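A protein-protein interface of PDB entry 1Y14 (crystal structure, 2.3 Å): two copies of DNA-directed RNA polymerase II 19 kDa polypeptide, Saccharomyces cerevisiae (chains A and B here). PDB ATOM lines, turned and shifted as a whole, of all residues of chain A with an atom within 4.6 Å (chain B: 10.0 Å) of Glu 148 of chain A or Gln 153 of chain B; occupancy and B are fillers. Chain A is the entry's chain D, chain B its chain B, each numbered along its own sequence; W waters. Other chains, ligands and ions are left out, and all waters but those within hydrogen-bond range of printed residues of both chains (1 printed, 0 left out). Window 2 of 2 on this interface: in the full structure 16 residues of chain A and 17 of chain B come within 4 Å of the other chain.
Ile 160 of chain A touches its own counterpart, Ile 160 of chain B.
2 positions are printed for both chains.
Of the 6 pairs that touch across the chains among the printed residues, 1 has its exchanged pair printed and touching as well.
The side-chain amide nitrogen (NE2) of Gln 153 of chain B sits close to the side-chain amino group (NZ) of Lys 164 of chain A, 2.8 Å away.
Hydrophobic or aromatic side chains of chain A that line the printed part of chain B: Leu 114 and Ile 160.
Hydrophobic or aromatic side chains of chain B that line the printed part of chain A: Ile 151 and Ile 160.
Among the printed residues, no Asp or Glu carboxylate lies within 4 Å of a Lys or Arg side-chain nitrogen of the other chain.
Lys 83 of chain A touches none of the printed residues of chain B.
Of chain B, only Ile 151 and Gln 153 come within 4 Å of Glu 148 of chain A.
No residue of chain B comes within 4 Å of Gly 149 of chain A.
No residue of chain B comes within 4 Å of Ser 162 of chain A.
Of the printed residues of chain B, Lys 164 of chain A touches Gln 153.
Of the printed residues of chain A, Ile 151 of chain B touches Glu 148 and Ile 160.
Gln 153 of chain B touches three residues of chain A.
Printed residues of chain A within 4 Å of Ile 160 of chain B: Ile 160 (3.6 Å).
The nearest residue of chain B that does not touch Glu 148 of chain A is Ser 152 of chain B (5.9 Å).
The nearest printed residue of chain A that does not touch Gln 153 of chain B is Ser 162 of chain A (4.9 Å).
The nearest printed residue of chain B that does not touch Ile 160 of chain A is His 158 of chain B (6.6 Å).
Among the printed residues, pairs that only touch across the chains: Ile 160 of chain A with Ile 160 of chain B, Leu 114 of chain A with Gln 153 of chain B, Ile 160 of chain A with Ile 151 of chain B, Glu 148 of chain A with Gln 153 of chain B and Glu 148 of chain A with Ile 151 of chain B.
The backbone carbonyl oxygen of Gly 149 of chain A is in hydrogen-bond range of the backbone NH of Ile 160 of chain A (2.8 Å).
The backbone carbonyl oxygen of Ile 151 of chain B is in hydrogen-bond range of the backbone NH of His 158 of chain B, at 2.7 Å.
The backbone NH (N) of Gly 40 of chain B sits close to the backbone carbonyl oxygen (O) of Gln 153 of chain B, 3.1 Å away.
The backbone NH of Ile 160 of chain B is in hydrogen-bond range of the backbone carbonyl oxygen of Gly 149 of chain B (2.9 Å).
OG of Ser 162 of chain A is in hydrogen-bond range of N of Lys 164 of chain A (3.1 Å).
N of Glu 148 of chain A is in hydrogen-bond range of O of Ile 160 of chain A (2.9 Å).
Water W1 lies within hydrogen-bond range of NE2 of Gln 153 of chain B (2.7 Å) and OG of Ser 162 of chain A (3.3 Å).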
ATOM      1  N   LYS A  83     -13.159  -5.965 -15.428  1.00  0.00           N
ATOM      2  CA  LYS A  83     -13.641  -6.024 -16.804  1.00  0.00           C
ATOM      3  C   LYS A  83     -15.040  -5.458 -16.878  1.00  0.00           C
ATOM      4  O   LYS A  83     -15.875  -5.782 -16.043  1.00  0.00           O
ATOM      5  CB  LYS A  83     -13.668  -7.470 -17.310  1.00  0.00           C
ATOM      6  CG  LYS A  83     -14.243  -7.612 -18.716  1.00  0.00           C
ATOM      7  CD  LYS A  83     -14.350  -9.074 -19.125  1.00  0.00           C
ATOM      8  CE  LYS A  83     -14.838  -9.219 -20.557  1.00  0.00           C
ATOM      9  NZ  LYS A  83     -14.926 -10.660 -20.943  1.00  0.00           N
ATOM     10  N   LEU A 114      -9.253  -0.884 -30.734  1.00  0.00           N
ATOM     11  CA  LEU A 114     -10.409  -0.733 -29.850  1.00  0.00           C
ATOM     12  C   LEU A 114     -10.932   0.696 -29.900  1.00  0.00           C
ATOM     13  O   LEU A 114     -11.558   1.182 -28.957  1.00  0.00           O
ATOM     14  CB  LEU A 114     -10.034  -1.126 -28.412  1.00  0.00           C
ATOM     15  CG  LEU A 114      -9.767  -2.625 -28.254  1.00  0.00           C
ATOM     16  CD1 LEU A 114      -9.178  -2.934 -26.891  1.00  0.00           C
ATOM     17  CD2 LEU A 114     -11.086  -3.380 -28.451  1.00  0.00           C
ATOM     18  N   LYS A 146     -13.826   2.022 -21.527  1.00  0.00           N
ATOM     19  CA  LYS A 146     -14.366   0.807 -20.942  1.00  0.00           C
ATOM     20  C   LYS A 146     -13.228  -0.158 -20.810  1.00  0.00           C
ATOM     21  O   LYS A 146     -12.509  -0.406 -21.770  1.00  0.00           O
ATOM     22  CB  LYS A 146     -15.441   0.188 -21.834  1.00  0.00           C
ATOM     23  CG  LYS A 146     -15.982  -1.142 -21.316  1.00  0.00           C
ATOM     24  CD  LYS A 146     -16.942  -1.766 -22.321  1.00  0.00           C
ATOM     25  CE  LYS A 146     -17.667  -2.976 -21.744  1.00  0.00           C
ATOM     26  NZ  LYS A 146     -18.566  -3.632 -22.745  1.00  0.00           N
ATOM     27  N   ILE A 147     -13.049  -0.702 -19.614  1.00  0.00           N
ATOM     28  CA  ILE A 147     -11.980  -1.664 -19.403  1.00  0.00           C
ATOM     29  C   ILE A 147     -12.445  -2.998 -19.992  1.00  0.00           C
ATOM     30  O   ILE A 147     -13.356  -3.642 -19.464  1.00  0.00           O
ATOM     31  CB  ILE A 147     -11.665  -1.805 -17.897  1.00  0.00           C
ATOM     32  CG1 ILE A 147     -11.137  -0.459 -17.368  1.00  0.00           C
ATOM     33  CG2 ILE A 147     -10.653  -2.941 -17.671  1.00  0.00           C
ATOM     34  CD1 ILE A 147     -10.913  -0.425 -15.878  1.00  0.00           C
ATOM     35  N   GLU A 148     -11.821  -3.384 -21.102  1.00  0.00           N
ATOM     36  CA  GLU A 148     -12.146  -4.623 -21.811  1.00  0.00           C
ATOM     37  C   GLU A 148     -11.461  -5.826 -21.188  1.00  0.00           C
ATOM     38  O   GLU A 148     -11.936  -6.955 -21.303  1.00  0.00           O
ATOM     39  CB  GLU A 148     -11.718  -4.525 -23.283  1.00  0.00           C
ATOM     40  CG  GLU A 148     -12.566  -3.593 -24.126  1.00  0.00           C
ATOM     41  CD  GLU A 148     -13.992  -4.073 -24.256  1.00  0.00           C
ATOM     42  OE1 GLU A 148     -14.218  -5.285 -24.068  1.00  0.00           O
ATOM     43  OE2 GLU A 148     -14.885  -3.249 -24.562  1.00  0.00           O
ATOM     44  N   GLY A 149     -10.336  -5.583 -20.534  1.00  0.00           N
ATOM     45  CA  GLY A 149      -9.620  -6.677 -19.922  1.00  0.00           C
ATOM     46  C   GLY A 149      -8.593  -6.227 -18.911  1.00  0.00           C
ATOM     47  O   GLY A 149      -8.039  -5.132 -19.016  1.00  0.00           O
ATOM     48  N   ILE A 160      -6.601  -3.036 -20.277  1.00  0.00           N
ATOM     49  CA  ILE A 160      -6.693  -2.727 -21.691  1.00  0.00           C
ATOM     50  C   ILE A 160      -8.086  -2.138 -21.864  1.00  0.00           C
ATOM     51  O   ILE A 160      -9.055  -2.701 -21.365  1.00  0.00           O
ATOM     52  CB  ILE A 160      -6.563  -3.994 -22.553  1.00  0.00           C
ATOM     53  CG1 ILE A 160      -5.215  -4.671 -22.291  1.00  0.00           C
ATOM     54  CG2 ILE A 160      -6.676  -3.628 -24.028  1.00  0.00           C
ATOM     55  CD1 ILE A 160      -4.032  -3.946 -22.899  1.00  0.00           C
ATOM     56  N   GLY A 161      -8.197  -1.014 -22.566  1.00  0.00           N
ATOM     57  CA  GLY A 161      -9.504  -0.398 -22.723  1.00  0.00           C
ATOM     58  C   GLY A 161      -9.990  -0.096 -24.124  1.00  0.00           C
ATOM     59  O   GLY A 161      -9.262  -0.221 -25.111  1.00  0.00           O
ATOM     60  N   SER A 162     -11.241   0.336 -24.191  1.00  0.00           N
ATOM     61  CA  SER A 162     -11.885   0.651 -25.440  1.00  0.00           C
ATOM     62  C   SER A 162     -12.754   1.903 -25.370  1.00  0.00           C
ATOM     63  O   SER A 162     -13.257   2.270 -24.309  1.00  0.00           O
ATOM     64  CB  SER A 162     -12.758  -0.539 -25.853  1.00  0.00           C
ATOM     65  OG  SER A 162     -13.894  -0.119 -26.594  1.00  0.00           O
ATOM     66  N   LYS A 164     -14.834   2.295 -28.299  1.00  0.00           N
ATOM     67  CA  LYS A 164     -15.641   1.979 -29.477  1.00  0.00           C
ATOM     68  C   LYS A 164     -17.145   2.114 -29.262  1.00  0.00           C
ATOM     69  O   LYS A 164     -17.851   2.656 -30.113  1.00  0.00           O
ATOM     70  CB  LYS A 164     -15.348   0.552 -29.951  1.00  0.00           C
ATOM     71  CG  LYS A 164     -14.262   0.439 -31.006  1.00  0.00           C
ATOM     72  CD  LYS A 164     -13.943  -1.024 -31.313  1.00  0.00           C
ATOM     73  CE  LYS A 164     -15.166  -1.781 -31.807  1.00  0.00           C
ATOM     74  NZ  LYS A 164     -14.883  -3.234 -32.000  1.00  0.00           N
ATOM     75  N   CYS B  38     -14.234 -13.525 -39.290  1.00  0.00           N
ATOM     76  CA  CYS B  38     -13.749 -13.665 -37.927  1.00  0.00           C
ATOM     77  C   CYS B  38     -14.847 -13.311 -36.949  1.00  0.00           C
ATOM     78  O   CYS B  38     -15.637 -12.395 -37.191  1.00  0.00           O
ATOM     79  CB  CYS B  38     -12.551 -12.748 -37.677  1.00  0.00           C
ATOM     80  SG  CYS B  38     -11.921 -12.814 -35.962  1.00  0.00           S
ATOM     81  N   THR B  39     -14.895 -14.044 -35.844  1.00  0.00           N
ATOM     82  CA  THR B  39     -15.887 -13.794 -34.809  1.00  0.00           C
ATOM     83  C   THR B  39     -15.239 -13.986 -33.453  1.00  0.00           C
ATOM     84  O   THR B  39     -14.301 -14.779 -33.313  1.00  0.00           O
ATOM     85  CB  THR B  39     -17.062 -14.768 -34.895  1.00  0.00           C
ATOM     86  OG1 THR B  39     -16.614 -16.084 -34.545  1.00  0.00           O
ATOM     87  CG2 THR B  39     -17.641 -14.775 -36.298  1.00  0.00           C
ATOM     88  N   GLY B  40     -15.745 -13.265 -32.456  1.00  0.00           N
ATOM     89  CA  GLY B  40     -15.207 -13.385 -31.113  1.00  0.00           C
ATOM     90  C   GLY B  40     -15.336 -14.814 -30.629  1.00  0.00           C
ATOM     91  O   GLY B  40     -14.389 -15.386 -30.098  1.00  0.00           O
ATOM     92  N   LYS B  41     -16.509 -15.401 -30.850  1.00  0.00           N
ATOM     93  CA  LYS B  41     -16.792 -16.770 -30.430  1.00  0.00           C
ATOM     94  C   LYS B  41     -15.920 -17.889 -30.990  1.00  0.00           C
ATOM     95  O   LYS B  41     -15.373 -18.681 -30.226  1.00  0.00           O
ATOM     96  CB  LYS B  41     -18.253 -17.119 -30.720  1.00  0.00           C
ATOM     97  CG  LYS B  41     -18.586 -18.583 -30.443  1.00  0.00           C
ATOM     98  CD  LYS B  41     -20.053 -18.884 -30.661  1.00  0.00           C
ATOM     99  CE  LYS B  41     -20.383 -20.314 -30.257  1.00  0.00           C
ATOM    100  NZ  LYS B  41     -21.843 -20.597 -30.385  1.00  0.00           N
ATOM    101  N   PHE B  42     -15.801 -17.974 -32.311  1.00  0.00           N
ATOM    102  CA  PHE B  42     -15.026 -19.050 -32.922  1.00  0.00           C
ATOM    103  C   PHE B  42     -13.613 -18.722 -33.359  1.00  0.00           C
ATOM    104  O   PHE B  42     -12.775 -19.616 -33.459  1.00  0.00           O
ATOM    105  CB  PHE B  42     -15.783 -19.632 -34.116  1.00  0.00           C
ATOM    106  CG  PHE B  42     -16.965 -20.470 -33.734  1.00  0.00           C
ATOM    107  CD1 PHE B  42     -16.795 -21.636 -32.987  1.00  0.00           C
ATOM    108  CD2 PHE B  42     -18.248 -20.106 -34.129  1.00  0.00           C
ATOM    109  CE1 PHE B  42     -17.885 -22.427 -32.641  1.00  0.00           C
ATOM    110  CE2 PHE B  42     -19.347 -20.891 -33.788  1.00  0.00           C
ATOM    111  CZ  PHE B  42     -19.165 -22.055 -33.042  1.00  0.00           C
ATOM    112  N   GLY B  43     -13.344 -17.454 -33.629  1.00  0.00           N
ATOM    113  CA  GLY B  43     -12.010 -17.078 -34.057  1.00  0.00           C
ATOM    114  C   GLY B  43     -12.001 -16.803 -35.544  1.00  0.00           C
ATOM    115  O   GLY B  43     -13.011 -16.393 -36.101  1.00  0.00           O
ATOM    116  N   TYR B  44     -10.865 -17.020 -36.192  1.00  0.00           N
ATOM    117  CA  TYR B  44     -10.781 -16.786 -37.624  1.00  0.00           C
ATOM    118  C   TYR B  44     -11.116 -18.046 -38.439  1.00  0.00           C
ATOM    119  O   TYR B  44     -10.510 -19.102 -38.238  1.00  0.00           O
ATOM    120  CB  TYR B  44      -9.378 -16.324 -38.016  1.00  0.00           C
ATOM    121  CG  TYR B  44      -8.924 -15.006 -37.446  1.00  0.00           C
ATOM    122  CD1 TYR B  44      -8.465 -14.906 -36.129  1.00  0.00           C
ATOM    123  CD2 TYR B  44      -8.872 -13.870 -38.249  1.00  0.00           C
ATOM    124  CE1 TYR B  44      -7.951 -13.712 -35.638  1.00  0.00           C
ATOM    125  CE2 TYR B  44      -8.359 -12.667 -37.765  1.00  0.00           C
ATOM    126  CZ  TYR B  44      -7.896 -12.598 -36.463  1.00  0.00           C
ATOM    127  OH  TYR B  44      -7.339 -11.431 -36.007  1.00  0.00           O
ATOM    128  N   LYS B  80      -7.742 -19.488 -33.181  1.00  0.00           N
ATOM    129  CA  LYS B  80      -8.218 -18.757 -32.009  1.00  0.00           C
ATOM    130  C   LYS B  80      -7.194 -18.873 -30.908  1.00  0.00           C
ATOM    131  O   LYS B  80      -6.837 -19.974 -30.478  1.00  0.00           O
ATOM    132  CB  LYS B  80      -9.544 -19.308 -31.500  1.00  0.00           C
ATOM    133  CG  LYS B  80     -10.227 -18.390 -30.486  1.00  0.00           C
ATOM    134  CD  LYS B  80     -11.418 -19.083 -29.835  1.00  0.00           C
ATOM    135  CE  LYS B  80     -12.064 -18.213 -28.765  1.00  0.00           C
ATOM    136  NZ  LYS B  80     -12.747 -17.029 -29.349  1.00  0.00           N
ATOM    137  N   GLY B 149      -3.820 -12.432 -22.381  1.00  0.00           N
ATOM    138  CA  GLY B 149      -5.223 -12.097 -22.426  1.00  0.00           C
ATOM    139  C   GLY B 149      -5.751 -12.020 -23.842  1.00  0.00           C
ATOM    140  O   GLY B 149      -5.021 -11.681 -24.769  1.00  0.00           O
ATOM    141  N   CYS B 150      -7.028 -12.346 -23.997  1.00  0.00           N
ATOM    142  CA  CYS B 150      -7.698 -12.309 -25.285  1.00  0.00           C
ATOM    143  C   CYS B 150      -8.943 -11.494 -25.102  1.00  0.00           C
ATOM    144  O   CYS B 150      -9.656 -11.650 -24.124  1.00  0.00           O
ATOM    145  CB  CYS B 150      -8.119 -13.707 -25.729  1.00  0.00           C
ATOM    146  SG  CYS B 150      -6.801 -14.913 -25.723  1.00  0.00           S
ATOM    147  N   ILE B 151      -9.207 -10.615 -26.047  1.00  0.00           N
ATOM    148  CA  ILE B 151     -10.397  -9.809 -25.975  1.00  0.00           C
ATOM    149  C   ILE B 151     -11.161 -10.119 -27.250  1.00  0.00           C
ATOM    150  O   ILE B 151     -10.658  -9.912 -28.353  1.00  0.00           O
ATOM    151  CB  ILE B 151     -10.031  -8.321 -25.885  1.00  0.00           C
ATOM    152  CG1 ILE B 151      -9.237  -8.076 -24.595  1.00  0.00           C
ATOM    153  CG2 ILE B 151     -11.287  -7.474 -25.886  1.00  0.00           C
ATOM    154  CD1 ILE B 151      -8.351  -6.854 -24.633  1.00  0.00           C
ATOM    155  N   SER B 152     -12.369 -10.649 -27.097  1.00  0.00           N
ATOM    156  CA  SER B 152     -13.172 -10.991 -28.255  1.00  0.00           C
ATOM    157  C   SER B 152     -14.348 -10.042 -28.450  1.00  0.00           C
ATOM    158  O   SER B 152     -15.213  -9.919 -27.585  1.00  0.00           O
ATOM    159  CB  SER B 152     -13.684 -12.424 -28.132  1.00  0.00           C
ATOM    160  OG  SER B 152     -14.651 -12.521 -27.106  1.00  0.00           O
ATOM    161  N   GLN B 153     -14.356  -9.363 -29.591  1.00  0.00           N
ATOM    162  CA  GLN B 153     -15.423  -8.440 -29.947  1.00  0.00           C
ATOM    163  C   GLN B 153     -16.337  -9.236 -30.882  1.00  0.00           C
ATOM    164  O   GLN B 153     -16.034 -10.379 -31.233  1.00  0.00           O
ATOM    165  CB  GLN B 153     -14.860  -7.225 -30.697  1.00  0.00           C
ATOM    166  CG  GLN B 153     -13.814  -6.378 -29.938  1.00  0.00           C
ATOM    167  CD  GLN B 153     -14.436  -5.374 -28.973  1.00  0.00           C
ATOM    168  OE1 GLN B 153     -14.844  -5.723 -27.863  1.00  0.00           O
ATOM    169  NE2 GLN B 153     -14.519  -4.121 -29.404  1.00  0.00           N
ATOM    170  N   VAL B 154     -17.443  -8.633 -31.301  1.00  0.00           N
ATOM    171  CA  VAL B 154     -18.380  -9.310 -32.192  1.00  0.00           C
ATOM    172  C   VAL B 154     -17.707  -9.891 -33.437  1.00  0.00           C
ATOM    173  O   VAL B 154     -17.954 -11.040 -33.812  1.00  0.00           O
ATOM    174  CB  VAL B 154     -19.514  -8.348 -32.638  1.00  0.00           C
ATOM    175  CG1 VAL B 154     -20.346  -8.985 -33.736  1.00  0.00           C
ATOM    176  CG2 VAL B 154     -20.399  -8.014 -31.450  1.00  0.00           C
ATOM    177  N   SER B 155     -16.853  -9.105 -34.077  1.00  0.00           N
ATOM    178  CA  SER B 155     -16.197  -9.582 -35.283  1.00  0.00           C
ATOM    179  C   SER B 155     -14.683  -9.412 -35.285  1.00  0.00           C
ATOM    180  O   SER B 155     -14.078  -9.049 -36.299  1.00  0.00           O
ATOM    181  CB  SER B 155     -16.810  -8.891 -36.499  1.00  0.00           C
ATOM    182  OG  SER B 155     -16.798  -7.491 -36.326  1.00  0.00           O
ATOM    183  N   SER B 156     -14.065  -9.699 -34.151  1.00  0.00           N
ATOM    184  CA  SER B 156     -12.618  -9.584 -34.048  1.00  0.00           C
ATOM    185  C   SER B 156     -12.122 -10.130 -32.719  1.00  0.00           C
ATOM    186  O   SER B 156     -12.905 -10.370 -31.798  1.00  0.00           O
ATOM    187  CB  SER B 156     -12.196  -8.118 -34.178  1.00  0.00           C
ATOM    188  OG  SER B 156     -12.750  -7.341 -33.128  1.00  0.00           O
ATOM    189  N   ILE B 157     -10.819 -10.344 -32.629  1.00  0.00           N
ATOM    190  CA  ILE B 157     -10.227 -10.821 -31.387  1.00  0.00           C
ATOM    191  C   ILE B 157      -8.896 -10.101 -31.213  1.00  0.00           C
ATOM    192  O   ILE B 157      -8.209  -9.799 -32.189  1.00  0.00           O
ATOM    193  CB  ILE B 157      -9.989 -12.346 -31.395  1.00  0.00           C
ATOM    194  CG1 ILE B 157      -9.085 -12.727 -32.562  1.00  0.00           C
ATOM    195  CG2 ILE B 157     -11.313 -13.086 -31.501  1.00  0.00           C
ATOM    196  CD1 ILE B 157      -8.756 -14.201 -32.602  1.00  0.00           C
ATOM    197  N   HIS B 158      -8.538  -9.820 -29.967  1.00  0.00           N
ATOM    198  CA  HIS B 158      -7.298  -9.120 -29.686  1.00  0.00           C
ATOM    199  C   HIS B 158      -6.529  -9.898 -28.654  1.00  0.00           C
ATOM    200  O   HIS B 158      -7.112 -10.520 -27.772  1.00  0.00           O
ATOM    201  CB  HIS B 158      -7.622  -7.719 -29.173  1.00  0.00           C
ATOM    202  CG  HIS B 158      -8.646  -7.020 -30.004  1.00  0.00           C
ATOM    203  ND1 HIS B 158      -8.315  -6.140 -31.010  1.00  0.00           N
ATOM    204  CD2 HIS B 158      -9.993  -7.146 -30.042  1.00  0.00           C
ATOM    205  CE1 HIS B 158      -9.414  -5.754 -31.634  1.00  0.00           C
ATOM    206  NE2 HIS B 158     -10.447  -6.350 -31.066  1.00  0.00           N
ATOM    207  N   ALA B 159      -5.212  -9.875 -28.767  1.00  0.00           N
ATOM    208  CA  ALA B 159      -4.403 -10.599 -27.816  1.00  0.00           C
ATOM    209  C   ALA B 159      -3.271  -9.749 -27.259  1.00  0.00           C
ATOM    210  O   ALA B 159      -2.661  -8.945 -27.972  1.00  0.00           O
ATOM    211  CB  ALA B 159      -3.845 -11.855 -28.467  1.00  0.00           C
ATOM    212  N   ILE B 160      -3.019  -9.912 -25.965  1.00  0.00           N
ATOM    213  CA  ILE B 160      -1.936  -9.209 -25.307  1.00  0.00           C
ATOM    214  C   ILE B 160      -0.914 -10.276 -24.922  1.00  0.00           C
ATOM    215  O   ILE B 160      -1.283 -11.358 -24.460  1.00  0.00           O
ATOM    216  CB  ILE B 160      -2.421  -8.477 -24.042  1.00  0.00           C
ATOM    217  CG1 ILE B 160      -3.550  -7.501 -24.394  1.00  0.00           C
ATOM    218  CG2 ILE B 160      -1.266  -7.746 -23.410  1.00  0.00           C
ATOM    219  CD1 ILE B 160      -3.168  -6.408 -25.407  1.00  0.00           C
HETATM  220  O   HOH W   1     -15.876  -2.276 -28.024  1.00  0.00           O
